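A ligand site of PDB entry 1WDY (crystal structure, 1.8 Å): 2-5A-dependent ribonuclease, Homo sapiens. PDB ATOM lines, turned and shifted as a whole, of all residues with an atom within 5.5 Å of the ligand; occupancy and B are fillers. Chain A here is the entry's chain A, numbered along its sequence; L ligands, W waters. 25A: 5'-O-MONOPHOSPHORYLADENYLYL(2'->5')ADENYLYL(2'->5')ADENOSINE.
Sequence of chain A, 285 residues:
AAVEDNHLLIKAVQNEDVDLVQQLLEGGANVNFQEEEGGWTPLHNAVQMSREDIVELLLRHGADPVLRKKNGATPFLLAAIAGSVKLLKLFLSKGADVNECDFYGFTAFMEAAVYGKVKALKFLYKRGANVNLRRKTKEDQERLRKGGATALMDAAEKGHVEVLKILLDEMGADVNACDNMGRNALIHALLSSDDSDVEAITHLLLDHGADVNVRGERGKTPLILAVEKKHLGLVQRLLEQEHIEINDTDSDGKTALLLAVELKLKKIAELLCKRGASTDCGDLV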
ATOM      1  N   GLN A  14       5.533   9.358  -0.209  1.00  0.00           N
ATOM      2  CA  GLN A  14       4.523   9.536   0.827  1.00  0.00           C
ATOM      3  C   GLN A  14       3.179   8.862   0.487  1.00  0.00           C
ATOM      4  O   GLN A  14       2.504   8.330   1.366  1.00  0.00           O
ATOM      5  CB  GLN A  14       4.322  11.036   1.116  1.00  0.00           C
ATOM      6  CG  GLN A  14       5.537  11.695   1.760  1.00  0.00           C
ATOM      7  CD  GLN A  14       5.433  13.205   1.912  1.00  0.00           C
ATOM      8  OE1 GLN A  14       4.677  13.863   1.193  1.00  0.00           O
ATOM      9  NE2 GLN A  14       6.194  13.756   2.844  1.00  0.00           N
ATOM     10  N   GLU A  35      13.725  18.533   1.174  1.00  0.00           N
ATOM     11  CA  GLU A  35      12.715  19.605   1.243  1.00  0.00           C
ATOM     12  C   GLU A  35      13.146  20.671   2.265  1.00  0.00           C
ATOM     13  O   GLU A  35      13.931  20.392   3.178  1.00  0.00           O
ATOM     14  CB  GLU A  35      11.302  19.055   1.493  1.00  0.00           C
ATOM     15  CG  GLU A  35      11.080  18.221   2.746  1.00  0.00           C
ATOM     16  CD  GLU A  35      11.034  19.053   4.007  1.00  0.00           C
ATOM     17  OE1 GLU A  35      11.693  18.672   4.995  1.00  0.00           O
ATOM     18  OE2 GLU A  35      10.322  20.083   4.033  1.00  0.00           O
ATOM     19  N   GLU A  37      11.763  22.820   4.590  1.00  0.00           N
ATOM     20  CA  GLU A  37      11.299  23.070   5.950  1.00  0.00           C
ATOM     21  C   GLU A  37      12.046  22.234   7.012  1.00  0.00           C
ATOM     22  O   GLU A  37      12.429  22.771   8.058  1.00  0.00           O
ATOM     23  CB  GLU A  37       9.779  22.844   6.042  1.00  0.00           C
ATOM     24  CG  GLU A  37       8.989  24.031   5.508  1.00  0.00           C
ATOM     25  CD  GLU A  37       7.858  23.672   4.546  1.00  0.00           C
ATOM     26  OE1 GLU A  37       7.358  24.589   3.859  1.00  0.00           O
ATOM     27  OE2 GLU A  37       7.466  22.489   4.489  1.00  0.00           O
ATOM     28  N   GLY A  38      12.253  20.953   6.734  1.00  0.00           N
ATOM     29  CA  GLY A  38      12.883  20.029   7.672  1.00  0.00           C
ATOM     30  C   GLY A  38      14.102  19.277   7.169  1.00  0.00           C
ATOM     31  O   GLY A  38      14.746  18.587   7.942  1.00  0.00           O
ATOM     32  N   TRP A  40      13.999  16.804   5.008  1.00  0.00           N
ATOM     33  CA  TRP A  40      13.611  15.407   4.781  1.00  0.00           C
ATOM     34  C   TRP A  40      13.888  14.996   3.352  1.00  0.00           C
ATOM     35  O   TRP A  40      13.713  15.765   2.433  1.00  0.00           O
ATOM     36  CB  TRP A  40      12.124  15.182   5.067  1.00  0.00           C
ATOM     37  CG  TRP A  40      11.765  15.213   6.521  1.00  0.00           C
ATOM     38  CD1 TRP A  40      11.780  16.301   7.338  1.00  0.00           C
ATOM     39  CD2 TRP A  40      11.338  14.106   7.327  1.00  0.00           C
ATOM     40  NE1 TRP A  40      11.384  15.948   8.611  1.00  0.00           N
ATOM     41  CE2 TRP A  40      11.115  14.603   8.624  1.00  0.00           C
ATOM     42  CE3 TRP A  40      11.107  12.745   7.083  1.00  0.00           C
ATOM     43  CZ2 TRP A  40      10.682  13.795   9.664  1.00  0.00           C
ATOM     44  CZ3 TRP A  40      10.703  11.945   8.122  1.00  0.00           C
ATOM     45  CH2 TRP A  40      10.484  12.471   9.399  1.00  0.00           C
ATOM     46  N   ASN A  45      11.360   9.708   4.379  1.00  0.00           N
ATOM     47  CA  ASN A  45       9.926   9.437   4.265  1.00  0.00           C
ATOM     48  C   ASN A  45       9.621   7.932   4.145  1.00  0.00           C
ATOM     49  O   ASN A  45       8.702   7.428   4.791  1.00  0.00           O
ATOM     50  CB  ASN A  45       9.349  10.227   3.071  1.00  0.00           C
ATOM     51  CG  ASN A  45       9.065  11.694   3.425  1.00  0.00           C
ATOM     52  OD1 ASN A  45       8.038  11.998   4.014  1.00  0.00           O
ATOM     53  ND2 ASN A  45       9.986  12.585   3.062  1.00  0.00           N
ATOM     54  N   GLN A  48      10.107   6.344   7.512  1.00  0.00           N
ATOM     55  CA  GLN A  48       9.042   6.760   8.435  1.00  0.00           C
ATOM     56  C   GLN A  48       7.782   5.915   8.247  1.00  0.00           C
ATOM     57  O   GLN A  48       7.039   5.644   9.218  1.00  0.00           O
ATOM     58  CB  GLN A  48       8.701   8.238   8.203  1.00  0.00           C
ATOM     59  CG  GLN A  48       7.617   8.762   9.124  1.00  0.00           C
ATOM     60  CD  GLN A  48       7.301  10.203   8.856  1.00  0.00           C
ATOM     61  OE1 GLN A  48       6.864  10.550   7.759  1.00  0.00           O
ATOM     62  NE2 GLN A  48       7.538  11.059   9.847  1.00  0.00           N
ATOM     63  N   LYS A  69      18.805  14.881   8.030  1.00  0.00           N
ATOM     64  CA  LYS A  69      17.920  16.030   7.848  1.00  0.00           C
ATOM     65  C   LYS A  69      18.315  17.134   8.856  1.00  0.00           C
ATOM     66  O   LYS A  69      19.344  17.019   9.521  1.00  0.00           O
ATOM     67  CB  LYS A  69      16.443  15.631   7.956  1.00  0.00           C
ATOM     68  CG  LYS A  69      16.039  14.788   9.143  1.00  0.00           C
ATOM     69  CD  LYS A  69      14.595  14.353   9.004  1.00  0.00           C
ATOM     70  CE  LYS A  69      14.155  13.515  10.185  1.00  0.00           C
ATOM     71  NZ  LYS A  69      14.042  14.290  11.446  1.00  0.00           N
ATOM     72  N   ASN A  71      17.394  18.310  11.792  1.00  0.00           N
ATOM     73  CA  ASN A  71      17.591  18.025  13.215  1.00  0.00           C
ATOM     74  C   ASN A  71      18.746  17.030  13.443  1.00  0.00           C
ATOM     75  O   ASN A  71      19.019  16.664  14.573  1.00  0.00           O
ATOM     76  CB  ASN A  71      16.301  17.540  13.879  1.00  0.00           C
ATOM     77  CG  ASN A  71      15.975  16.076  13.597  1.00  0.00           C
ATOM     78  OD1 ASN A  71      16.279  15.549  12.524  1.00  0.00           O
ATOM     79  ND2 ASN A  71      15.350  15.417  14.560  1.00  0.00           N
ATOM     80  N   ILE A  81      12.419   5.053  15.589  1.00  0.00           N
ATOM     81  CA  ILE A  81      11.110   5.647  15.817  1.00  0.00           C
ATOM     82  C   ILE A  81       9.985   4.763  15.240  1.00  0.00           C
ATOM     83  O   ILE A  81       8.956   4.576  15.882  1.00  0.00           O
ATOM     84  CB  ILE A  81      11.054   7.077  15.263  1.00  0.00           C
ATOM     85  CG1 ILE A  81      11.981   7.985  16.089  1.00  0.00           C
ATOM     86  CG2 ILE A  81       9.606   7.620  15.281  1.00  0.00           C
ATOM     87  CD1 ILE A  81      12.115   9.398  15.594  1.00  0.00           C
ATOM     88  N   ASP A 102      21.213  12.368  16.854  1.00  0.00           N
ATOM     89  CA  ASP A 102      20.846  13.601  16.190  1.00  0.00           C
ATOM     90  C   ASP A 102      21.431  14.795  16.942  1.00  0.00           C
ATOM     91  O   ASP A 102      22.200  14.626  17.908  1.00  0.00           O
ATOM     92  CB  ASP A 102      19.333  13.677  15.953  1.00  0.00           C
ATOM     93  CG  ASP A 102      18.515  13.918  17.221  1.00  0.00           C
ATOM     94  OD1 ASP A 102      19.073  14.351  18.258  1.00  0.00           O
ATOM     95  OD2 ASP A 102      17.279  13.710  17.250  1.00  0.00           O
ATOM     96  N   TYR A 104      20.198  16.996  18.862  1.00  0.00           N
ATOM     97  CA  TYR A 104      19.712  17.190  20.235  1.00  0.00           C
ATOM     98  C   TYR A 104      20.090  16.027  21.154  1.00  0.00           C
ATOM     99  O   TYR A 104      19.704  15.972  22.336  1.00  0.00           O
ATOM    100  CB  TYR A 104      18.196  17.451  20.206  1.00  0.00           C
ATOM    101  CG  TYR A 104      17.883  18.796  19.587  1.00  0.00           C
ATOM    102  CD1 TYR A 104      17.879  19.956  20.366  1.00  0.00           C
ATOM    103  CD2 TYR A 104      17.666  18.918  18.219  1.00  0.00           C
ATOM    104  CE1 TYR A 104      17.621  21.201  19.789  1.00  0.00           C
ATOM    105  CE2 TYR A 104      17.424  20.165  17.624  1.00  0.00           C
ATOM    106  CZ  TYR A 104      17.396  21.305  18.422  1.00  0.00           C
ATOM    107  OH  TYR A 104      17.158  22.541  17.846  1.00  0.00           O
ATOM    108  N   PHE A 106      19.587  12.592  20.644  1.00  0.00           N
ATOM    109  CA  PHE A 106      18.790  11.367  20.600  1.00  0.00           C
ATOM    110  C   PHE A 106      19.471  10.246  19.823  1.00  0.00           C
ATOM    111  O   PHE A 106      19.801  10.407  18.665  1.00  0.00           O
ATOM    112  CB  PHE A 106      17.409  11.618  20.000  1.00  0.00           C
ATOM    113  CG  PHE A 106      16.482  12.346  20.933  1.00  0.00           C
ATOM    114  CD1 PHE A 106      15.675  11.654  21.806  1.00  0.00           C
ATOM    115  CD2 PHE A 106      16.474  13.734  20.954  1.00  0.00           C
ATOM    116  CE1 PHE A 106      14.830  12.339  22.677  1.00  0.00           C
ATOM    117  CE2 PHE A 106      15.650  14.410  21.827  1.00  0.00           C
ATOM    118  CZ  PHE A 106      14.830  13.711  22.682  1.00  0.00           C
ATOM    119  N   GLU A 111      15.194   6.634  21.104  1.00  0.00           N
ATOM    120  CA  GLU A 111      13.988   6.787  20.310  1.00  0.00           C
ATOM    121  C   GLU A 111      13.092   5.570  20.483  1.00  0.00           C
ATOM    122  O   GLU A 111      11.871   5.701  20.544  1.00  0.00           O
ATOM    123  CB  GLU A 111      14.294   7.021  18.822  1.00  0.00           C
ATOM    124  CG  GLU A 111      14.946   8.359  18.471  1.00  0.00           C
ATOM    125  CD  GLU A 111      14.049   9.582  18.718  1.00  0.00           C
ATOM    126  OE1 GLU A 111      12.980   9.455  19.340  1.00  0.00           O
ATOM    127  OE2 GLU A 111      14.431  10.697  18.291  1.00  0.00           O
ATOM    128  N   VAL A 114      11.416   6.155  23.790  1.00  0.00           N
ATOM    129  CA  VAL A 114      10.407   7.223  23.662  1.00  0.00           C
ATOM    130  C   VAL A 114       9.124   6.674  23.038  1.00  0.00           C
ATOM    131  O   VAL A 114       8.018   6.983  23.508  1.00  0.00           O
ATOM    132  CB  VAL A 114      10.931   8.410  22.770  1.00  0.00           C
ATOM    133  CG1 VAL A 114       9.812   9.360  22.336  1.00  0.00           C
ATOM    134  CG2 VAL A 114      12.014   9.183  23.504  1.00  0.00           C
ATOM    135  N   TYR A 115       9.272   5.846  22.008  1.00  0.00           N
ATOM    136  CA  TYR A 115       8.133   5.393  21.203  1.00  0.00           C
ATOM    137  C   TYR A 115       7.637   3.998  21.612  1.00  0.00           C
ATOM    138  O   TYR A 115       6.751   3.439  20.961  1.00  0.00           O
ATOM    139  CB  TYR A 115       8.477   5.465  19.712  1.00  0.00           C
ATOM    140  CG  TYR A 115       8.407   6.882  19.195  1.00  0.00           C
ATOM    141  CD1 TYR A 115       7.198   7.446  18.799  1.00  0.00           C
ATOM    142  CD2 TYR A 115       9.544   7.701  19.180  1.00  0.00           C
ATOM    143  CE1 TYR A 115       7.121   8.751  18.359  1.00  0.00           C
ATOM    144  CE2 TYR A 115       9.467   9.018  18.753  1.00  0.00           C
ATOM    145  CZ  TYR A 115       8.250   9.539  18.333  1.00  0.00           C
ATOM    146  OH  TYR A 115       8.148  10.832  17.881  1.00  0.00           O
ATOM    147  N   ARG A 135      22.015  12.629  26.806  1.00  0.00           N
ATOM    148  CA  ARG A 135      21.921  13.379  25.567  1.00  0.00           C
ATOM    149  C   ARG A 135      22.915  14.539  25.532  1.00  0.00           C
ATOM    150  O   ARG A 135      22.958  15.356  26.437  1.00  0.00           O
ATOM    151  CB  ARG A 135      20.502  13.899  25.341  1.00  0.00           C
ATOM    152  CG  ARG A 135      19.548  12.824  24.889  1.00  0.00           C
ATOM    153  CD  ARG A 135      18.342  13.346  24.138  1.00  0.00           C
ATOM    154  NE  ARG A 135      17.200  13.681  24.986  1.00  0.00           N
ATOM    155  CZ  ARG A 135      16.413  12.790  25.576  1.00  0.00           C
ATOM    156  NH1 ARG A 135      16.665  11.491  25.462  1.00  0.00           N
ATOM    157  NH2 ARG A 135      15.361  13.192  26.263  1.00  0.00           N
ATOM    158  N   LYS A 146      19.607  22.395  29.348  1.00  0.00           N
ATOM    159  CA  LYS A 146      18.908  21.344  28.616  1.00  0.00           C
ATOM    160  C   LYS A 146      19.900  20.235  28.266  1.00  0.00           C
ATOM    161  O   LYS A 146      21.120  20.418  28.383  1.00  0.00           O
ATOM    162  CB  LYS A 146      18.241  21.895  27.356  1.00  0.00           C
ATOM    163  CG  LYS A 146      17.342  23.088  27.633  1.00  0.00           C
ATOM    164  CD  LYS A 146      15.997  23.003  26.925  1.00  0.00           C
ATOM    165  CE  LYS A 146      15.057  24.119  27.373  1.00  0.00           C
ATOM    166  NZ  LYS A 146      15.453  25.423  26.777  1.00  0.00           N
ATOM    167  N   GLY A 147      19.377  19.094  27.843  1.00  0.00           N
ATOM    168  CA  GLY A 147      20.219  17.949  27.552  1.00  0.00           C
ATOM    169  C   GLY A 147      20.451  17.066  28.761  1.00  0.00           C
ATOM    170  O   GLY A 147      19.997  17.356  29.870  1.00  0.00           O
ATOM    171  N   GLY A 148      21.146  15.960  28.526  1.00  0.00           N
ATOM    172  CA  GLY A 148      21.586  15.066  29.570  1.00  0.00           C
ATOM    173  C   GLY A 148      20.638  13.931  29.905  1.00  0.00           C
ATOM    174  O   GLY A 148      20.957  13.110  30.746  1.00  0.00           O
ATOM    175  N   ALA A 149      19.475  13.878  29.265  1.00  0.00           N
ATOM    176  CA  ALA A 149      18.505  12.818  29.575  1.00  0.00           C
ATOM    177  C   ALA A 149      18.902  11.467  28.979  1.00  0.00           C
ATOM    178  O   ALA A 149      19.686  11.390  28.028  1.00  0.00           O
ATOM    179  CB  ALA A 149      17.106  13.210  29.119  1.00  0.00           C
ATOM    180  N   ASP A 154      13.130   8.850  29.325  1.00  0.00           N
ATOM    181  CA  ASP A 154      12.125   8.923  28.273  1.00  0.00           C
ATOM    182  C   ASP A 154      11.009   7.900  28.496  1.00  0.00           C
ATOM    183  O   ASP A 154       9.817   8.195  28.291  1.00  0.00           O
ATOM    184  CB  ASP A 154      12.724   8.642  26.896  1.00  0.00           C
ATOM    185  CG  ASP A 154      13.738   9.674  26.478  1.00  0.00           C
ATOM    186  OD1 ASP A 154      13.518  10.891  26.721  1.00  0.00           O
ATOM    187  OD2 ASP A 154      14.781   9.339  25.879  1.00  0.00           O
ATOM    188  N   GLU A 157       8.866   9.245  31.400  1.00  0.00           N
ATOM    189  CA  GLU A 157       8.089  10.400  30.954  1.00  0.00           C
ATOM    190  C   GLU A 157       6.890   9.990  30.081  1.00  0.00           C
ATOM    191  O   GLU A 157       5.786  10.508  30.258  1.00  0.00           O
ATOM    192  CB  GLU A 157       8.987  11.356  30.172  1.00  0.00           C
ATOM    193  CG  GLU A 157       8.405  12.746  29.933  1.00  0.00           C
ATOM    194  CD  GLU A 157       9.056  13.465  28.759  1.00  0.00           C
ATOM    195  OE1 GLU A 157       8.314  14.029  27.914  1.00  0.00           O
ATOM    196  OE2 GLU A 157      10.312  13.481  28.667  1.00  0.00           O
HETATM  197  O1P 25A L   1      14.906  18.122  26.355  1.00  0.00           O
HETATM  198  P   25A L   1      15.081  16.879  25.538  1.00  0.00           P
HETATM  199  O2P 25A L   1      16.544  16.418  25.642  1.00  0.00           O
HETATM  200  O3P 25A L   1      14.074  15.816  26.004  1.00  0.00           O
HETATM  201  O5' 25A L   1      14.703  17.287  24.042  1.00  0.00           O
HETATM  202  C5' 25A L   1      15.510  18.170  23.322  1.00  0.00           C
HETATM  203  C4' 25A L   1      14.755  18.664  22.093  1.00  0.00           C
HETATM  204  O4' 25A L   1      14.693  17.711  21.038  1.00  0.00           O
HETATM  205  C1' 25A L   1      13.426  17.772  20.390  1.00  0.00           C
HETATM  206  C2' 25A L   1      12.744  18.959  21.022  1.00  0.00           C
HETATM  207  O2' 25A L   1      13.124  20.120  20.340  1.00  0.00           O
HETATM  208  C3' 25A L   1      13.331  19.053  22.400  1.00  0.00           C
HETATM  209  O3' 25A L   1      13.200  20.353  22.944  1.00  0.00           O
HETATM  210  N9  25A L   1      12.771  16.486  20.683  1.00  0.00           N
HETATM  211  C8  25A L   1      11.868  16.178  21.662  1.00  0.00           C
HETATM  212  N7  25A L   1      11.605  14.857  21.588  1.00  0.00           N
HETATM  213  C5  25A L   1      12.339  14.313  20.594  1.00  0.00           C
HETATM  214  C6  25A L   1      12.466  13.008  20.096  1.00  0.00           C
HETATM  215  N6  25A L   1      11.777  11.987  20.597  1.00  0.00           N
HETATM  216  C4  25A L   1      13.091  15.332  20.022  1.00  0.00           C
HETATM  217  N3  25A L   1      13.928  15.124  18.990  1.00  0.00           N
HETATM  218  C2  25A L   1      14.059  13.840  18.504  1.00  0.00           C
HETATM  219  N1  25A L   1      13.328  12.807  19.032  1.00  0.00           N
HETATM  220  P1  25A L   1      12.247  20.996  19.294  1.00  0.00           P
HETATM  221  OBP 25A L   1      10.821  20.915  19.657  1.00  0.00           O
HETATM  222  OCP 25A L   1      13.022  22.244  19.088  1.00  0.00           O
HETATM  223  OF' 25A L   1      12.381  20.127  17.947  1.00  0.00           O
HETATM  224  CF' 25A L   1      13.566  20.064  17.156  1.00  0.00           C
HETATM  225  CE' 25A L   1      13.301  19.059  16.061  1.00  0.00           C
HETATM  226  OE' 25A L   1      13.232  17.722  16.636  1.00  0.00           O
HETATM  227  CB' 25A L   1      12.270  16.962  15.939  1.00  0.00           C
HETATM  228  N19 25A L   1      11.320  16.467  16.916  1.00  0.00           N
HETATM  229  C18 25A L   1      10.593  17.178  17.829  1.00  0.00           C
HETATM  230  N17 25A L   1       9.824  16.426  18.591  1.00  0.00           N
HETATM  231  C15 25A L   1      10.064  15.138  18.134  1.00  0.00           C
HETATM  232  C14 25A L   1      10.973  15.150  17.097  1.00  0.00           C
HETATM  233  N13 25A L   1      11.450  14.099  16.426  1.00  0.00           N
HETATM  234  C12 25A L   1      10.916  12.957  16.869  1.00  0.00           C
HETATM  235  N11 25A L   1      10.014  12.793  17.853  1.00  0.00           N
HETATM  236  C16 25A L   1       9.563  13.876  18.517  1.00  0.00           C
HETATM  237  N16 25A L   1       8.673  13.717  19.497  1.00  0.00           N
HETATM  238  CC' 25A L   1      11.680  17.857  14.861  1.00  0.00           C
HETATM  239  OC' 25A L   1      12.378  17.633  13.657  1.00  0.00           O
HETATM  240  CD' 25A L   1      11.972  19.254  15.346  1.00  0.00           C
HETATM  241  OD' 25A L   1      12.105  20.165  14.259  1.00  0.00           O
HETATM  242  P2  25A L   1      11.571  16.792  12.427  1.00  0.00           P
HETATM  243  OLP 25A L   1      12.579  16.525  11.382  1.00  0.00           O
HETATM  244  OMP 25A L   1      10.796  15.711  13.067  1.00  0.00           O
HETATM  245  OP' 25A L   1      10.467  17.851  11.934  1.00  0.00           O
HETATM  246  CP' 25A L   1      10.865  19.130  11.444  1.00  0.00           C
HETATM  247  CO' 25A L   1       9.939  19.638  10.354  1.00  0.00           C
HETATM  248  OO' 25A L   1      10.049  18.794   9.185  1.00  0.00           O
HETATM  249  CL' 25A L   1       8.881  18.964   8.399  1.00  0.00           C
HETATM  250  N29 25A L   1       8.619  17.694   7.741  1.00  0.00           N
HETATM  251  C28 25A L   1       8.837  17.430   6.418  1.00  0.00           C
HETATM  252  N27 25A L   1       8.540  16.214   6.087  1.00  0.00           N
HETATM  253  C25 25A L   1       8.083  15.636   7.240  1.00  0.00           C
HETATM  254  C24 25A L   1       8.123  16.532   8.286  1.00  0.00           C
HETATM  255  N23 25A L   1       7.749  16.300   9.552  1.00  0.00           N
HETATM  256  C22 25A L   1       7.327  15.050   9.707  1.00  0.00           C
HETATM  257  N21 25A L   1       7.242  14.085   8.792  1.00  0.00           N
HETATM  258  C26 25A L   1       7.612  14.340   7.519  1.00  0.00           C
HETATM  259  N26 25A L   1       7.527  13.376   6.603  1.00  0.00           N
HETATM  260  CM' 25A L   1       7.767  19.470   9.330  1.00  0.00           C
HETATM  261  OM' 25A L   1       7.254  20.686   8.836  1.00  0.00           O
HETATM  262  CN' 25A L   1       8.457  19.602  10.681  1.00  0.00           C
HETATM  263  ON' 25A L   1       8.093  20.789  11.364  1.00  0.00           O
HETATM  264  O   HOH W   1      11.706  13.190  13.244  1.00  0.00           O
HETATM  265  O   HOH W   2      17.850  16.032  27.830  1.00  0.00           O
HETATM  266  O   HOH W   3      15.979  16.154  17.152  1.00  0.00           O
HETATM  267  O   HOH W   4       7.673  12.016  21.688  1.00  0.00           O
HETATM  268  O   HOH W   5       7.516  15.827  16.113  1.00  0.00           O
HETATM  269  O   HOH W   6      11.736  15.113  25.197  1.00  0.00           O
HETATM  270  O   HOH W   7       6.158  17.299  12.042  1.00  0.00           O
HETATM  271  O   HOH W   8       4.388  12.847   9.199  1.00  0.00           O
HETATM  272  O   HOH W   9      16.374  18.966  28.397  1.00  0.00           O
HETATM  273  O   HOH W  10      14.548  18.063  10.694  1.00  0.00           O
HETATM  274  O   HOH W  11      14.170  20.147  12.261  1.00  0.00           O
HETATM  275  O   HOH W  12       8.950  15.247   3.489  1.00  0.00           O
HETATM  276  O   HOH W  13      13.881  15.216  28.669  1.00  0.00           O
HETATM  277  O   HOH W  14      13.967  20.737  25.534  1.00  0.00           O
HETATM  278  O   HOH W  15      18.681  17.394  24.449  1.00  0.00           O
HETATM  279  O   HOH W  16      10.391  12.861  23.138  1.00  0.00           O
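Glu 35 touches the ligand. CA of Gly 38 touches OO' of the ligand, 3.4 Å away. Asn 71 touches the ligand (ND2 to CB', 3.7 Å). Ile 81 touches the ligand. Asp 102 touches the ligand (OD2 to C2, 3.5 Å). Tyr 104 touches the ligand. CE2 of Phe 106 touches C4 of the ligand, at 3.3 Å. CG1 of Val 114 touches N6 of the ligand, at 3.7 Å. 15 residues have an atom within 4 Å of the ligand: Glu 35, Gly 38, Trp 40, Asn 45, Gln 48, Lys 69, Asn 71, Ile 81, Asp 102, Tyr 104, Phe 106, Glu 111, Val 114, Tyr 115 and Arg 135.
A nitrogen (N1) of the ligand sits at hydrogen-bond distance from the side-chain carboxylate (OE2) of Glu 111 (2.5 Å). An oxygen (OLP) of the ligand is in salt-bridge range of the side-chain amino group (NZ) of Lys 69 (2.7 Å). A nitrogen (N11) of the ligand lies within hydrogen-bond range of the side-chain hydroxyl (OH) of Tyr 115, at 2.7 Å. NE of Arg 135 is in salt-bridge range of O2P of the ligand, at 2.9 Å. N26 of the ligand lies within hydrogen-bond range of OD1 of Asn 45 (3.0 Å). An oxygen (OLP) of the ligand is in hydrogen-bond range of the indole nitrogen (NE1) of Trp 40 (3.1 Å). OE1 of Gln 48 sits at hydrogen-bond distance from N26 of the ligand.
Water W10 lies within hydrogen-bond range of an oxygen (OLP) of the ligand (2.6 Å), the backbone carbonyl oxygen (O) of Gly 38 (2.8 Å) and the backbone NH (N) of Asn 71 (3.1 Å). Water W15 bridges an oxygen (O2P) of the ligand (2.6 Å) and the backbone carbonyl oxygen of Tyr 104 (2.7 Å). Water W1 bridges an oxygen (OMP) of the ligand (2.7 Å) and the side-chain amino group (NZ) of Lys 69 (3.1 Å). Water W13 bridges an oxygen (O3P) of the ligand and the guanidinium group of Arg 135. Water W12 lies within hydrogen-bond range of a nitrogen (N27) of the ligand (2.8 Å), the side-chain amide nitrogen of Asn 45 (2.9 Å) and the side-chain amide nitrogen of Gln 14 (3.2 Å). Water W3 lies within hydrogen-bond range of ND2 of Asn 71 (2.8 Å), OD2 of Asp 102 (2.8 Å) and N3 of the ligand (2.9 Å).
The side-chain amino group (NZ) of Lys 69 sits at hydrogen-bond distance from the side-chain amide oxygen (OD1) of Asn 71 (2.8 Å). The guanidinium group (NH1) of Arg 135 lies within salt-bridge range of the side-chain carboxylate (OD2) of Asp 154, at 2.9 Å. The backbone NH (N) of Gly 148 sits at hydrogen-bond distance from the backbone carbonyl oxygen (O) of Arg 135 (2.8 Å). The side-chain amide oxygen (OD1) of Asn 45 lies within hydrogen-bond range of the side-chain amide nitrogen (NE2) of Gln 14 (2.8 Å). N of Trp 40 lies within hydrogen-bond range of OE1 of Glu 35, at 3.0 Å. The backbone NH (N) of Phe 106 is in hydrogen-bond range of the side-chain carboxylate (OD1) of Asp 102 (3.0 Å). The side-chain carboxylate of Glu 35 sits at hydrogen-bond distance from the backbone NH of Gly 38, 2.9 Å away. OE2 of Glu 35 is in hydrogen-bond range of N of Glu 37 (3.1 Å).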
